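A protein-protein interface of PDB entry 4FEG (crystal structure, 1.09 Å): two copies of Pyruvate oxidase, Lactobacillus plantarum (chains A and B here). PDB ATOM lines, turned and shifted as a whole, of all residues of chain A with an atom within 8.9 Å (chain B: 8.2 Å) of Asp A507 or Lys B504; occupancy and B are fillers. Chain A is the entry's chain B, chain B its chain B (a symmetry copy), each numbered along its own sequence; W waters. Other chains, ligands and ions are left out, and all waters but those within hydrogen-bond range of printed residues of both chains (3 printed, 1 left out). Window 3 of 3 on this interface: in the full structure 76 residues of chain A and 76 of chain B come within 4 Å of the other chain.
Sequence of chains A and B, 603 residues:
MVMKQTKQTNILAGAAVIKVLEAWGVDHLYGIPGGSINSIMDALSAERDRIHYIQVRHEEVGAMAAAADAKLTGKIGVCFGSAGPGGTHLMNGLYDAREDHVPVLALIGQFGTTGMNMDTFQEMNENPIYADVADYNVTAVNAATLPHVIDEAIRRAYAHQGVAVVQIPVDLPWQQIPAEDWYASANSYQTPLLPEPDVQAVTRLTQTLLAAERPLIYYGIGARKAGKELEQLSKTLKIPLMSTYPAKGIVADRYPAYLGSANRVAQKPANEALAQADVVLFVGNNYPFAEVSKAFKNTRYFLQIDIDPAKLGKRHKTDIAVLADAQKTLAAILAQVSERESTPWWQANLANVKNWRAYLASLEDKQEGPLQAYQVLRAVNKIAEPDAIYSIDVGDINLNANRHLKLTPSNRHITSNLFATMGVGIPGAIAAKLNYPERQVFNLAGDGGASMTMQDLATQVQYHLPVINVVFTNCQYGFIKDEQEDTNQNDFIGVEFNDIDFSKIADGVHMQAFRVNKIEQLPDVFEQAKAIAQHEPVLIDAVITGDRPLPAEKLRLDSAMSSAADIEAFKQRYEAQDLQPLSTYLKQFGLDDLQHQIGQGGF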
ATOM      1  N   MET A 454     -16.664 -11.003  -3.380  1.00  0.00           N
ATOM      2  CA  MET A 454     -16.855 -10.512  -2.063  1.00  0.00           C
ATOM      3  C   MET A 454     -16.971 -11.599  -1.018  1.00  0.00           C
ATOM      4  O   MET A 454     -16.650 -11.427   0.160  1.00  0.00           O
ATOM      5  CB  MET A 454     -18.141  -9.640  -1.952  1.00  0.00           C
ATOM      6  CG  MET A 454     -19.439 -10.331  -2.302  1.00  0.00           C
ATOM      7  SD  MET A 454     -21.036  -9.604  -1.810  1.00  0.00           S
ATOM      8  CE  MET A 454     -20.852  -8.042  -2.575  1.00  0.00           C
ATOM      9  N   LEU A 457     -14.051 -12.454   1.228  1.00  0.00           N
ATOM     10  CA  LEU A 457     -13.706 -11.741   2.447  1.00  0.00           C
ATOM     11  C   LEU A 457     -13.801 -12.650   3.660  1.00  0.00           C
ATOM     12  O   LEU A 457     -13.034 -12.524   4.621  1.00  0.00           O
ATOM     13  CB  LEU A 457     -14.585 -10.519   2.622  1.00  0.00           C
ATOM     14  CG  LEU A 457     -14.368  -9.405   1.585  1.00  0.00           C
ATOM     15  CD1 LEU A 457     -15.492  -8.377   1.677  1.00  0.00           C
ATOM     16  CD2 LEU A 457     -13.033  -8.719   1.766  1.00  0.00           C
ATOM     17  N   VAL A 461     -11.177 -13.665   7.051  1.00  0.00           N
ATOM     18  CA  VAL A 461     -11.570 -13.819   8.452  1.00  0.00           C
ATOM     19  C   VAL A 461     -11.241 -15.219   8.984  1.00  0.00           C
ATOM     20  O   VAL A 461     -10.665 -15.374  10.026  1.00  0.00           O
ATOM     21  CB  VAL A 461     -13.084 -13.537   8.576  1.00  0.00           C
ATOM     22  CG1 VAL A 461     -13.579 -13.816   9.999  1.00  0.00           C
ATOM     23  CG2 VAL A 461     -13.373 -12.069   8.200  1.00  0.00           C
ATOM     24  N   ILE A 500     -23.807  -0.949  -3.112  1.00  0.00           N
ATOM     25  CA  ILE A 500     -23.583  -1.981  -2.108  1.00  0.00           C
ATOM     26  C   ILE A 500     -22.742  -1.373  -0.995  1.00  0.00           C
ATOM     27  O   ILE A 500     -21.722  -0.762  -1.255  1.00  0.00           O
ATOM     28  CB  ILE A 500     -22.913  -3.248  -2.692  1.00  0.00           C
ATOM     29  CG1 ILE A 500     -23.788  -3.896  -3.730  1.00  0.00           C
ATOM     30  CG2 ILE A 500     -22.496  -4.184  -1.531  1.00  0.00           C
ATOM     31  CD1 ILE A 500     -23.226  -5.132  -4.420  1.00  0.00           C
ATOM     32  N   ASP A 501     -23.189  -1.517   0.247  1.00  0.00           N
ATOM     33  CA  ASP A 501     -22.435  -1.042   1.395  1.00  0.00           C
ATOM     34  C   ASP A 501     -21.491  -2.158   1.862  1.00  0.00           C
ATOM     35  O   ASP A 501     -21.888  -3.102   2.518  1.00  0.00           O
ATOM     36  CB  ASP A 501     -23.355  -0.537   2.477  1.00  0.00           C
ATOM     37  CG  ASP A 501     -22.684   0.002   3.701  1.00  0.00           C
ATOM     38  OD1 ASP A 501     -21.488  -0.286   3.913  1.00  0.00           O
ATOM     39  OD2 ASP A 501     -23.388   0.697   4.490  1.00  0.00           O
ATOM     40  N   PHE A 502     -20.224  -2.033   1.447  1.00  0.00           N
ATOM     41  CA  PHE A 502     -19.245  -3.060   1.764  1.00  0.00           C
ATOM     42  C   PHE A 502     -18.902  -3.067   3.249  1.00  0.00           C
ATOM     43  O   PHE A 502     -18.362  -4.078   3.705  1.00  0.00           O
ATOM     44  CB  PHE A 502     -17.984  -2.961   0.892  1.00  0.00           C
ATOM     45  CG  PHE A 502     -18.127  -3.668  -0.391  1.00  0.00           C
ATOM     46  CD1 PHE A 502     -17.712  -4.966  -0.459  1.00  0.00           C
ATOM     47  CD2 PHE A 502     -18.645  -2.990  -1.474  1.00  0.00           C
ATOM     48  CE1 PHE A 502     -17.836  -5.666  -1.696  1.00  0.00           C
ATOM     49  CE2 PHE A 502     -18.785  -3.621  -2.676  1.00  0.00           C
ATOM     50  CZ  PHE A 502     -18.373  -4.951  -2.760  1.00  0.00           C
ATOM     51  N   SER A 503     -19.181  -2.000   4.003  1.00  0.00           N
ATOM     52  CA  SER A 503     -18.991  -2.118   5.432  1.00  0.00           C
ATOM     53  C   SER A 503     -19.966  -3.105   6.018  1.00  0.00           C
ATOM     54  O   SER A 503     -19.625  -3.790   6.997  1.00  0.00           O
ATOM     55  CB  SER A 503     -19.009  -0.747   6.109  1.00  0.00           C
ATOM     56  OG  SER A 503     -20.286  -0.193   6.296  1.00  0.00           O
ATOM     57  N   LYS A 504     -21.179  -3.186   5.458  1.00  0.00           N
ATOM     58  CA  LYS A 504     -22.172  -4.138   5.918  1.00  0.00           C
ATOM     59  C   LYS A 504     -21.881  -5.547   5.429  1.00  0.00           C
ATOM     60  O   LYS A 504     -22.082  -6.529   6.123  1.00  0.00           O
ATOM     61  CB  LYS A 504     -23.585  -3.687   5.482  1.00  0.00           C
ATOM     62  CG  LYS A 504     -24.057  -2.447   6.226  1.00  0.00           C
ATOM     63  CD  LYS A 504     -25.428  -1.994   5.740  1.00  0.00           C
ATOM     64  CE  LYS A 504     -25.955  -0.908   6.678  1.00  0.00           C
ATOM     65  NZ  LYS A 504     -27.262  -0.438   6.277  1.00  0.00           N
ATOM     66  N   ILE A 505     -21.361  -5.675   4.199  1.00  0.00           N
ATOM     67  CA  ILE A 505     -20.877  -6.943   3.715  1.00  0.00           C
ATOM     68  C   ILE A 505     -19.794  -7.478   4.648  1.00  0.00           C
ATOM     69  O   ILE A 505     -19.839  -8.656   5.060  1.00  0.00           O
ATOM     70  CB  ILE A 505     -20.364  -6.846   2.280  1.00  0.00           C
ATOM     71  CG1 ILE A 505     -21.401  -6.362   1.248  1.00  0.00           C
ATOM     72  CG2 ILE A 505     -19.745  -8.171   1.805  1.00  0.00           C
ATOM     73  CD1 ILE A 505     -22.629  -7.217   1.138  1.00  0.00           C
ATOM     74  N   ALA A 506     -18.850  -6.621   4.979  1.00  0.00           N
ATOM     75  CA  ALA A 506     -17.797  -6.998   5.917  1.00  0.00           C
ATOM     76  C   ALA A 506     -18.340  -7.453   7.248  1.00  0.00           C
ATOM     77  O   ALA A 506     -17.953  -8.485   7.798  1.00  0.00           O
ATOM     78  CB  ALA A 506     -16.798  -5.858   6.085  1.00  0.00           C
ATOM     79  N   ASP A 507     -19.286  -6.666   7.788  1.00  0.00           N
ATOM     80  CA  ASP A 507     -19.934  -7.085   9.028  1.00  0.00           C
ATOM     81  C   ASP A 507     -20.553  -8.469   8.889  1.00  0.00           C
ATOM     82  O   ASP A 507     -20.437  -9.307   9.797  1.00  0.00           O
ATOM     83  CB  ASP A 507     -20.973  -6.054   9.420  1.00  0.00           C
ATOM     84  CG  ASP A 507     -21.559  -6.232  10.824  1.00  0.00           C
ATOM     85  OD1 ASP A 507     -21.122  -6.987  11.675  1.00  0.00           O
ATOM     86  OD2 ASP A 507     -22.572  -5.502  11.044  1.00  0.00           O
ATOM     87  N   GLY A 508     -21.189  -8.748   7.781  1.00  0.00           N
ATOM     88  CA  GLY A 508     -21.782 -10.035   7.530  1.00  0.00           C
ATOM     89  C   GLY A 508     -20.812 -11.201   7.552  1.00  0.00           C
ATOM     90  O   GLY A 508     -21.178 -12.304   7.976  1.00  0.00           O
ATOM     91  N   VAL A 509     -19.565 -10.986   7.121  1.00  0.00           N
ATOM     92  CA  VAL A 509     -18.544 -12.032   7.211  1.00  0.00           C
ATOM     93  C   VAL A 509     -17.687 -11.934   8.471  1.00  0.00           C
ATOM     94  O   VAL A 509     -16.729 -12.677   8.637  1.00  0.00           O
ATOM     95  CB  VAL A 509     -17.650 -12.090   5.936  1.00  0.00           C
ATOM     96  CG1 VAL A 509     -18.475 -12.213   4.673  1.00  0.00           C
ATOM     97  CG2 VAL A 509     -16.712 -10.868   5.852  1.00  0.00           C
ATOM     98  N   HIS A 510     -18.093 -11.013   9.356  1.00  0.00           N
ATOM     99  CA  HIS A 510     -17.471 -10.841  10.656  1.00  0.00           C
ATOM    100  C   HIS A 510     -16.076 -10.224  10.571  1.00  0.00           C
ATOM    101  O   HIS A 510     -15.152 -10.627  11.290  1.00  0.00           O
ATOM    102  CB  HIS A 510     -17.501 -12.144  11.521  1.00  0.00           C
ATOM    103  CG  HIS A 510     -18.857 -12.751  11.489  1.00  0.00           C
ATOM    104  ND1 HIS A 510     -19.982 -12.049  11.855  1.00  0.00           N
ATOM    105  CD2 HIS A 510     -19.289 -13.956  11.080  1.00  0.00           C
ATOM    106  CE1 HIS A 510     -21.046 -12.819  11.704  1.00  0.00           C
ATOM    107  NE2 HIS A 510     -20.653 -13.992  11.222  1.00  0.00           N
ATOM    108  N   MET A 511     -15.953  -9.223   9.732  1.00  0.00           N
ATOM    109  CA  MET A 511     -14.749  -8.389   9.537  1.00  0.00           C
ATOM    110  C   MET A 511     -15.049  -6.975   9.982  1.00  0.00           C
ATOM    111  O   MET A 511     -16.070  -6.404   9.550  1.00  0.00           O
ATOM    112  CB  MET A 511     -14.346  -8.417   8.079  1.00  0.00           C
ATOM    113  CG  MET A 511     -13.106  -7.581   7.765  1.00  0.00           C
ATOM    114  SD  MET A 511     -12.670  -7.564   6.021  1.00  0.00           S
ATOM    115  CE  MET A 511     -12.467  -9.338   5.715  1.00  0.00           C
ATOM    116  N   GLN A 512     -14.183  -6.349  10.747  1.00  0.00           N
ATOM    117  CA  GLN A 512     -14.305  -4.954  11.111  1.00  0.00           C
ATOM    118  C   GLN A 512     -14.220  -4.086   9.865  1.00  0.00           C
ATOM    119  O   GLN A 512     -13.459  -4.339   8.933  1.00  0.00           O
ATOM    120  CB  GLN A 512     -13.198  -4.548  12.090  1.00  0.00           C
ATOM    121  CG  GLN A 512     -13.372  -5.129  13.475  1.00  0.00           C
ATOM    122  CD  GLN A 512     -12.460  -4.349  14.451  1.00  0.00           C
ATOM    123  OE1 GLN A 512     -11.593  -5.032  14.957  1.00  0.00           O
ATOM    124  NE2 GLN A 512     -12.691  -3.077  14.632  1.00  0.00           N
ATOM    125  N   ALA A 513     -14.992  -3.002   9.844  1.00  0.00           N
ATOM    126  CA  ALA A 513     -15.073  -2.170   8.646  1.00  0.00           C
ATOM    127  C   ALA A 513     -15.583  -0.761   8.944  1.00  0.00           C
ATOM    128  O   ALA A 513     -16.178  -0.486   9.987  1.00  0.00           O
ATOM    129  CB  ALA A 513     -15.948  -2.808   7.592  1.00  0.00           C
ATOM    130  N   PHE A 514     -15.358   0.096   7.956  1.00  0.00           N
ATOM    131  CA  PHE A 514     -15.734   1.489   8.002  1.00  0.00           C
ATOM    132  C   PHE A 514     -16.267   1.862   6.622  1.00  0.00           C
ATOM    133  O   PHE A 514     -15.804   1.347   5.613  1.00  0.00           O
ATOM    134  CB  PHE A 514     -14.501   2.399   8.256  1.00  0.00           C
ATOM    135  CG  PHE A 514     -13.762   1.995   9.506  1.00  0.00           C
ATOM    136  CD1 PHE A 514     -12.798   1.014   9.513  1.00  0.00           C
ATOM    137  CD2 PHE A 514     -14.064   2.635  10.693  1.00  0.00           C
ATOM    138  CE1 PHE A 514     -12.158   0.629  10.667  1.00  0.00           C
ATOM    139  CE2 PHE A 514     -13.434   2.256  11.897  1.00  0.00           C
ATOM    140  CZ  PHE A 514     -12.489   1.253  11.854  1.00  0.00           C
ATOM    141  N   LEU A 539     -11.838  -3.616   6.454  1.00  0.00           N
ATOM    142  CA  LEU A 539     -12.275  -3.099   5.181  1.00  0.00           C
ATOM    143  C   LEU A 539     -12.702  -1.647   5.368  1.00  0.00           C
ATOM    144  O   LEU A 539     -13.406  -1.260   6.320  1.00  0.00           O
ATOM    145  CB  LEU A 539     -13.423  -3.938   4.609  1.00  0.00           C
ATOM    146  CG  LEU A 539     -13.952  -3.552   3.244  1.00  0.00           C
ATOM    147  CD1 LEU A 539     -14.376  -4.775   2.447  1.00  0.00           C
ATOM    148  CD2 LEU A 539     -15.081  -2.515   3.320  1.00  0.00           C
ATOM    149  N   LEU B 457     -27.756 -10.868  -5.119  1.00  0.00           N
ATOM    150  CA  LEU B 457     -28.874 -10.330  -4.359  1.00  0.00           C
ATOM    151  C   LEU B 457     -29.118  -8.871  -4.701  1.00  0.00           C
ATOM    152  O   LEU B 457     -30.258  -8.393  -4.706  1.00  0.00           O
ATOM    153  CB  LEU B 457     -28.643 -10.502  -2.871  1.00  0.00           C
ATOM    154  CG  LEU B 457     -28.650 -11.956  -2.373  1.00  0.00           C
ATOM    155  CD1 LEU B 457     -28.119 -12.023  -0.944  1.00  0.00           C
ATOM    156  CD2 LEU B 457     -30.032 -12.566  -2.433  1.00  0.00           C
ATOM    157  N   ASP B 499     -19.267 -18.867   9.948  1.00  0.00           N
ATOM    158  CA  ASP B 499     -20.522 -18.251   9.689  1.00  0.00           C
ATOM    159  C   ASP B 499     -20.400 -17.036   8.781  1.00  0.00           C
ATOM    160  O   ASP B 499     -19.501 -16.229   8.917  1.00  0.00           O
ATOM    161  CB  ASP B 499     -21.122 -17.806  11.008  1.00  0.00           C
ATOM    162  CG  ASP B 499     -22.457 -17.152  10.902  1.00  0.00           C
ATOM    163  OD1 ASP B 499     -23.458 -17.871  10.741  1.00  0.00           O
ATOM    164  OD2 ASP B 499     -22.541 -15.942  10.924  1.00  0.00           O
ATOM    165  N   ILE B 500     -21.386 -16.888   7.902  1.00  0.00           N
ATOM    166  CA  ILE B 500     -21.743 -15.641   7.240  1.00  0.00           C
ATOM    167  C   ILE B 500     -23.172 -15.297   7.633  1.00  0.00           C
ATOM    168  O   ILE B 500     -24.056 -16.129   7.543  1.00  0.00           O
ATOM    169  CB  ILE B 500     -21.585 -15.715   5.701  1.00  0.00           C
ATOM    170  CG1 ILE B 500     -20.154 -15.968   5.313  1.00  0.00           C
ATOM    171  CG2 ILE B 500     -22.207 -14.447   5.066  1.00  0.00           C
ATOM    172  CD1 ILE B 500     -19.867 -16.108   3.824  1.00  0.00           C
ATOM    173  N   ASP B 501     -23.391 -14.073   8.101  1.00  0.00           N
ATOM    174  CA  ASP B 501     -24.726 -13.608   8.440  1.00  0.00           C
ATOM    175  C   ASP B 501     -25.365 -12.986   7.191  1.00  0.00           C
ATOM    176  O   ASP B 501     -25.076 -11.867   6.813  1.00  0.00           O
ATOM    177  CB  ASP B 501     -24.691 -12.680   9.627  1.00  0.00           C
ATOM    178  CG  ASP B 501     -26.017 -12.158  10.083  1.00  0.00           C
ATOM    179  OD1 ASP B 501     -26.994 -12.225   9.309  1.00  0.00           O
ATOM    180  OD2 ASP B 501     -26.068 -11.628  11.232  1.00  0.00           O
ATOM    181  N   PHE B 502     -26.215 -13.787   6.537  1.00  0.00           N
ATOM    182  CA  PHE B 502     -26.835 -13.341   5.299  1.00  0.00           C
ATOM    183  C   PHE B 502     -27.855 -12.237   5.551  1.00  0.00           C
ATOM    184  O   PHE B 502     -28.197 -11.547   4.587  1.00  0.00           O
ATOM    185  CB  PHE B 502     -27.441 -14.500   4.494  1.00  0.00           C
ATOM    186  CG  PHE B 502     -26.456 -15.157   3.619  1.00  0.00           C
ATOM    187  CD1 PHE B 502     -26.344 -14.714   2.333  1.00  0.00           C
ATOM    188  CD2 PHE B 502     -25.711 -16.203   4.118  1.00  0.00           C
ATOM    189  CE1 PHE B 502     -25.400 -15.342   1.467  1.00  0.00           C
ATOM    190  CE2 PHE B 502     -24.793 -16.832   3.326  1.00  0.00           C
ATOM    191  CZ  PHE B 502     -24.660 -16.386   2.012  1.00  0.00           C
ATOM    192  N   SER B 503     -28.349 -12.052   6.778  1.00  0.00           N
ATOM    193  CA  SER B 503     -29.183 -10.892   7.000  1.00  0.00           C
ATOM    194  C   SER B 503     -28.379  -9.626   6.856  1.00  0.00           C
ATOM    195  O   SER B 503     -28.929  -8.604   6.410  1.00  0.00           O
ATOM    196  CB  SER B 503     -29.944 -10.999   8.322  1.00  0.00           C
ATOM    197  OG  SER B 503     -29.187 -10.711   9.469  1.00  0.00           O
ATOM    198  N   LYS B 504     -27.098  -9.658   7.238  1.00  0.00           N
ATOM    199  CA  LYS B 504     -26.228  -8.504   7.095  1.00  0.00           C
ATOM    200  C   LYS B 504     -25.768  -8.312   5.659  1.00  0.00           C
ATOM    201  O   LYS B 504     -25.643  -7.206   5.161  1.00  0.00           O
ATOM    202  CB  LYS B 504     -25.016  -8.630   8.047  1.00  0.00           C
ATOM    203  CG  LYS B 504     -25.405  -8.476   9.509  1.00  0.00           C
ATOM    204  CD  LYS B 504     -24.202  -8.656  10.427  1.00  0.00           C
ATOM    205  CE  LYS B 504     -24.595  -8.252  11.848  1.00  0.00           C
ATOM    206  NZ  LYS B 504     -23.492  -8.392  12.771  1.00  0.00           N
ATOM    207  N   ILE B 505     -25.527  -9.417   4.938  1.00  0.00           N
ATOM    208  CA  ILE B 505     -25.270  -9.349   3.521  1.00  0.00           C
ATOM    209  C   ILE B 505     -26.440  -8.674   2.811  1.00  0.00           C
ATOM    210  O   ILE B 505     -26.237  -7.752   1.994  1.00  0.00           O
ATOM    211  CB  ILE B 505     -24.992 -10.728   2.927  1.00  0.00           C
ATOM    212  CG1 ILE B 505     -23.794 -11.474   3.545  1.00  0.00           C
ATOM    213  CG2 ILE B 505     -24.830 -10.668   1.400  1.00  0.00           C
ATOM    214  CD1 ILE B 505     -22.479 -10.759   3.434  1.00  0.00           C
ATOM    215  N   ALA B 506     -27.637  -9.119   3.130  1.00  0.00           N
ATOM    216  CA  ALA B 506     -28.836  -8.507   2.565  1.00  0.00           C
ATOM    217  C   ALA B 506     -28.924  -7.029   2.852  1.00  0.00           C
ATOM    218  O   ALA B 506     -29.184  -6.204   1.977  1.00  0.00           O
ATOM    219  CB  ALA B 506     -30.086  -9.241   3.040  1.00  0.00           C
ATOM    220  N   ASP B 507     -28.685  -6.671   4.125  1.00  0.00           N
ATOM    221  CA  ASP B 507     -28.655  -5.252   4.469  1.00  0.00           C
ATOM    222  C   ASP B 507     -27.647  -4.497   3.613  1.00  0.00           C
ATOM    223  O   ASP B 507     -27.931  -3.387   3.134  1.00  0.00           O
ATOM    224  CB  ASP B 507     -28.344  -5.103   5.944  1.00  0.00           C
ATOM    225  CG  ASP B 507     -28.523  -3.687   6.501  1.00  0.00           C
ATOM    226  OD1 ASP B 507     -29.062  -2.767   5.912  1.00  0.00           O
ATOM    227  OD2 ASP B 507     -28.050  -3.540   7.668  1.00  0.00           O
ATOM    228  N   GLY B 508     -26.490  -5.062   3.384  1.00  0.00           N
ATOM    229  CA  GLY B 508     -25.479  -4.453   2.562  1.00  0.00           C
ATOM    230  C   GLY B 508     -25.899  -4.177   1.130  1.00  0.00           C
ATOM    231  O   GLY B 508     -25.468  -3.180   0.539  1.00  0.00           O
ATOM    232  N   VAL B 509     -26.753  -5.029   0.554  1.00  0.00           N
ATOM    233  CA  VAL B 509     -27.287  -4.772  -0.785  1.00  0.00           C
ATOM    234  C   VAL B 509     -28.640  -4.066  -0.771  1.00  0.00           C
ATOM    235  O   VAL B 509     -29.259  -3.874  -1.811  1.00  0.00           O
ATOM    236  CB  VAL B 509     -27.346  -6.066  -1.651  1.00  0.00           C
ATOM    237  CG1 VAL B 509     -26.009  -6.773  -1.701  1.00  0.00           C
ATOM    238  CG2 VAL B 509     -28.446  -7.026  -1.152  1.00  0.00           C
ATOM    239  N   HIS B 510     -29.052  -3.662   0.439  1.00  0.00           N
ATOM    240  CA  HIS B 510     -30.261  -2.885   0.642  1.00  0.00           C
ATOM    241  C   HIS B 510     -31.535  -3.697   0.419  1.00  0.00           C
ATOM    242  O   HIS B 510     -32.511  -3.210  -0.166  1.00  0.00           O
ATOM    243  CB  HIS B 510     -30.257  -1.538  -0.154  1.00  0.00           C
ATOM    244  CG  HIS B 510     -28.958  -0.839   0.024  1.00  0.00           C
ATOM    245  ND1 HIS B 510     -28.461  -0.524   1.268  1.00  0.00           N
ATOM    246  CD2 HIS B 510     -28.022  -0.450  -0.858  1.00  0.00           C
ATOM    247  CE1 HIS B 510     -27.285   0.065   1.132  1.00  0.00           C
ATOM    248  NE2 HIS B 510     -26.986   0.116  -0.161  1.00  0.00           N
ATOM    249  N   MET B 511     -31.530  -4.905   0.930  1.00  0.00           N
ATOM    250  CA  MET B 511     -32.665  -5.851   0.947  1.00  0.00           C
ATOM    251  C   MET B 511     -33.096  -6.080   2.378  1.00  0.00           C
ATOM    252  O   MET B 511     -32.240  -6.385   3.232  1.00  0.00           O
ATOM    253  CB  MET B 511     -32.247  -7.154   0.300  1.00  0.00           C
ATOM    254  CG  MET B 511     -33.351  -8.209   0.267  1.00  0.00           C
ATOM    255  SD  MET B 511     -32.830  -9.777  -0.444  1.00  0.00           S
ATOM    256  CE  MET B 511     -32.275  -9.229  -2.079  1.00  0.00           C
ATOM    257  N   ALA B 513     -34.335  -8.139   5.546  1.00  0.00           N
ATOM    258  CA  ALA B 513     -33.932  -9.494   5.917  1.00  0.00           C
ATOM    259  C   ALA B 513     -34.119  -9.772   7.408  1.00  0.00           C
ATOM    260  O   ALA B 513     -34.253  -8.868   8.233  1.00  0.00           O
ATOM    261  CB  ALA B 513     -32.496  -9.764   5.534  1.00  0.00           C
ATOM    262  N   PHE B 514     -34.075 -11.064   7.707  1.00  0.00           N
ATOM    263  CA  PHE B 514     -34.239 -11.584   9.044  1.00  0.00           C
ATOM    264  C   PHE B 514     -33.234 -12.720   9.216  1.00  0.00           C
ATOM    265  O   PHE B 514     -32.937 -13.439   8.272  1.00  0.00           O
ATOM    266  CB  PHE B 514     -35.647 -12.210   9.239  1.00  0.00           C
ATOM    267  CG  PHE B 514     -36.741 -11.231   8.900  1.00  0.00           C
ATOM    268  CD1 PHE B 514     -37.208 -11.055   7.618  1.00  0.00           C
ATOM    269  CD2 PHE B 514     -37.298 -10.479   9.916  1.00  0.00           C
ATOM    270  CE1 PHE B 514     -38.180 -10.132   7.317  1.00  0.00           C
ATOM    271  CE2 PHE B 514     -38.289  -9.514   9.639  1.00  0.00           C
ATOM    272  CZ  PHE B 514     -38.710  -9.362   8.335  1.00  0.00           C
ATOM    273  N   ARG B 515     -32.818 -12.953  10.465  1.00  0.00           N
ATOM    274  CA  ARG B 515     -32.069 -14.150  10.835  1.00  0.00           C
ATOM    275  C   ARG B 515     -32.791 -14.831  11.973  1.00  0.00           C
ATOM    276  O   ARG B 515     -33.198 -14.161  12.937  1.00  0.00           O
ATOM    277  CB  ARG B 515     -30.629 -13.816  11.225  1.00  0.00           C
ATOM    278  CG  ARG B 515     -29.806 -15.018  11.648  1.00  0.00           C
ATOM    279  CD  ARG B 515     -28.335 -14.703  11.782  1.00  0.00           C
ATOM    280  NE  ARG B 515     -27.558 -15.361  10.811  1.00  0.00           N
ATOM    281  CZ  ARG B 515     -26.395 -15.971  10.999  1.00  0.00           C
ATOM    282  NH1 ARG B 515     -25.882 -16.590   9.965  1.00  0.00           N
ATOM    283  NH2 ARG B 515     -25.752 -16.004  12.139  1.00  0.00           N
ATOM    284  N   LEU B 539     -34.971 -11.604   2.479  1.00  0.00           N
ATOM    285  CA  LEU B 539     -34.143 -12.753   2.751  1.00  0.00           C
ATOM    286  C   LEU B 539     -34.355 -13.170   4.203  1.00  0.00           C
ATOM    287  O   LEU B 539     -34.391 -12.359   5.147  1.00  0.00           O
ATOM    288  CB  LEU B 539     -32.666 -12.447   2.479  1.00  0.00           C
ATOM    289  CG  LEU B 539     -31.678 -13.578   2.665  1.00  0.00           C
ATOM    290  CD1 LEU B 539     -30.548 -13.499   1.652  1.00  0.00           C
ATOM    291  CD2 LEU B 539     -31.138 -13.661   4.100  1.00  0.00           C
ATOM    292  N   ASP B 541     -32.399 -15.754   6.781  1.00  0.00           N
ATOM    293  CA  ASP B 541     -31.219 -16.554   7.047  1.00  0.00           C
ATOM    294  C   ASP B 541     -31.567 -17.477   8.207  1.00  0.00           C
ATOM    295  O   ASP B 541     -31.712 -17.055   9.357  1.00  0.00           O
ATOM    296  CB  ASP B 541     -30.032 -15.655   7.391  1.00  0.00           C
ATOM    297  CG  ASP B 541     -28.742 -16.430   7.546  1.00  0.00           C
ATOM    298  OD1 ASP B 541     -28.759 -17.597   7.176  1.00  0.00           O
ATOM    299  OD2 ASP B 541     -27.725 -15.784   7.930  1.00  0.00           O
HETATM  300  O   HOH W   1     -28.633  -1.417   9.202  1.00  0.00           O
HETATM  301  O   HOH W   2     -23.086 -14.650  13.406  1.00  0.00           O
HETATM  302  O   HOH W   3     -23.550  -5.098  13.510  1.00  0.00           O
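Asp A501 touches Gly B508, and with the chains exchanged Gly A508 touches Asp B501. Lys A504 touches its own counterpart, Lys B504. Lys A504 touches Asp B507, and with the chains exchanged Asp A507 touches Lys B504. Ile B505 touches its own counterpart, Ile A505.
Printed residues of chain A that touch a printed residue of chain B: Ile A500, Asp A501, Lys A504, Ile A505, Asp A507, Gly A508 and His A510. Along chain A the printed residues that touch a printed residue of chain B span positions 500 to 510. Of the 19 printed residues of chain B, 7 touch a printed residue of chain A. Among the printed residues, Asp or Glu carboxylates within 4 Å of a Lys or Arg side-chain nitrogen of the other chain: Lys A504 with Asp B507 and Asp A507 with Lys B504.
CA of Ile A500 touches O of Gly B508, at 3.5 Å. O of Lys B504 touches O of Lys A504 (3.8 Å). CB of Lys A504 touches CA of Gly B508, 3.6 Å away. Ile B505 touches Ile A505. CA of Ile B500 touches O of Gly A508, at 3.5 Å. CA of Gly A508 touches CB of Lys B504 (3.6 Å).
The side-chain carboxylate (OD2) of Asp B499 lies within hydrogen-bond range of the backbone NH (N) of Asp B501. NH1 of Arg B515 sits at hydrogen-bond distance from O of Ile B500 (3.1 Å).
Printed residues of chain B within 4 Å of Asp A501: Gly B508. Phe A502 touches none of the printed residues of chain B. Of the printed residues of chain B, Asp A507 touches Lys B504. Of chain B, only Ile B500, Asp B501 and Lys B504 come within 4 Å of Gly A508. Of chain A, only Lys A504 (3.8 Å), Asp A507 (3.0 Å) and Gly A508 (3.6 Å) come within 4 Å of Lys B504. Printed residues of chain A within 4 Å of Asp B507: Lys A504. The nearest residue of chain B that does not touch Asp A507 is Asp B501 (5.4 Å). The nearest residue of chain A that does not touch Lys B504 is Ile A505 (4.6 Å).
Water W3 bridges OD2 of Asp A507 (2.7 Å) and NZ of Lys B504 (3.4 Å). Water W2 lies within hydrogen-bond range of OD2 of Asp B499 (2.9 Å), NH2 of Arg B515 (3.2 Å) and NE2 of His A510 (3.3 Å).
N of Asp A501 sits at hydrogen-bond distance from O of Gly B508. NZ of Lys A504 lies within salt-bridge range of OD1 of Asp B507 (3.0 Å). The side-chain amino group of Lys B504 is in salt-bridge range of the side-chain carboxylate of Asp A507 (3.0 Å). O of Gly A508 sits at hydrogen-bond distance from N of Asp B501. A ring nitrogen (NE2) of His A510 is in hydrogen-bond range of the side-chain carboxylate (OD2) of Asp B499 (2.7 Å).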
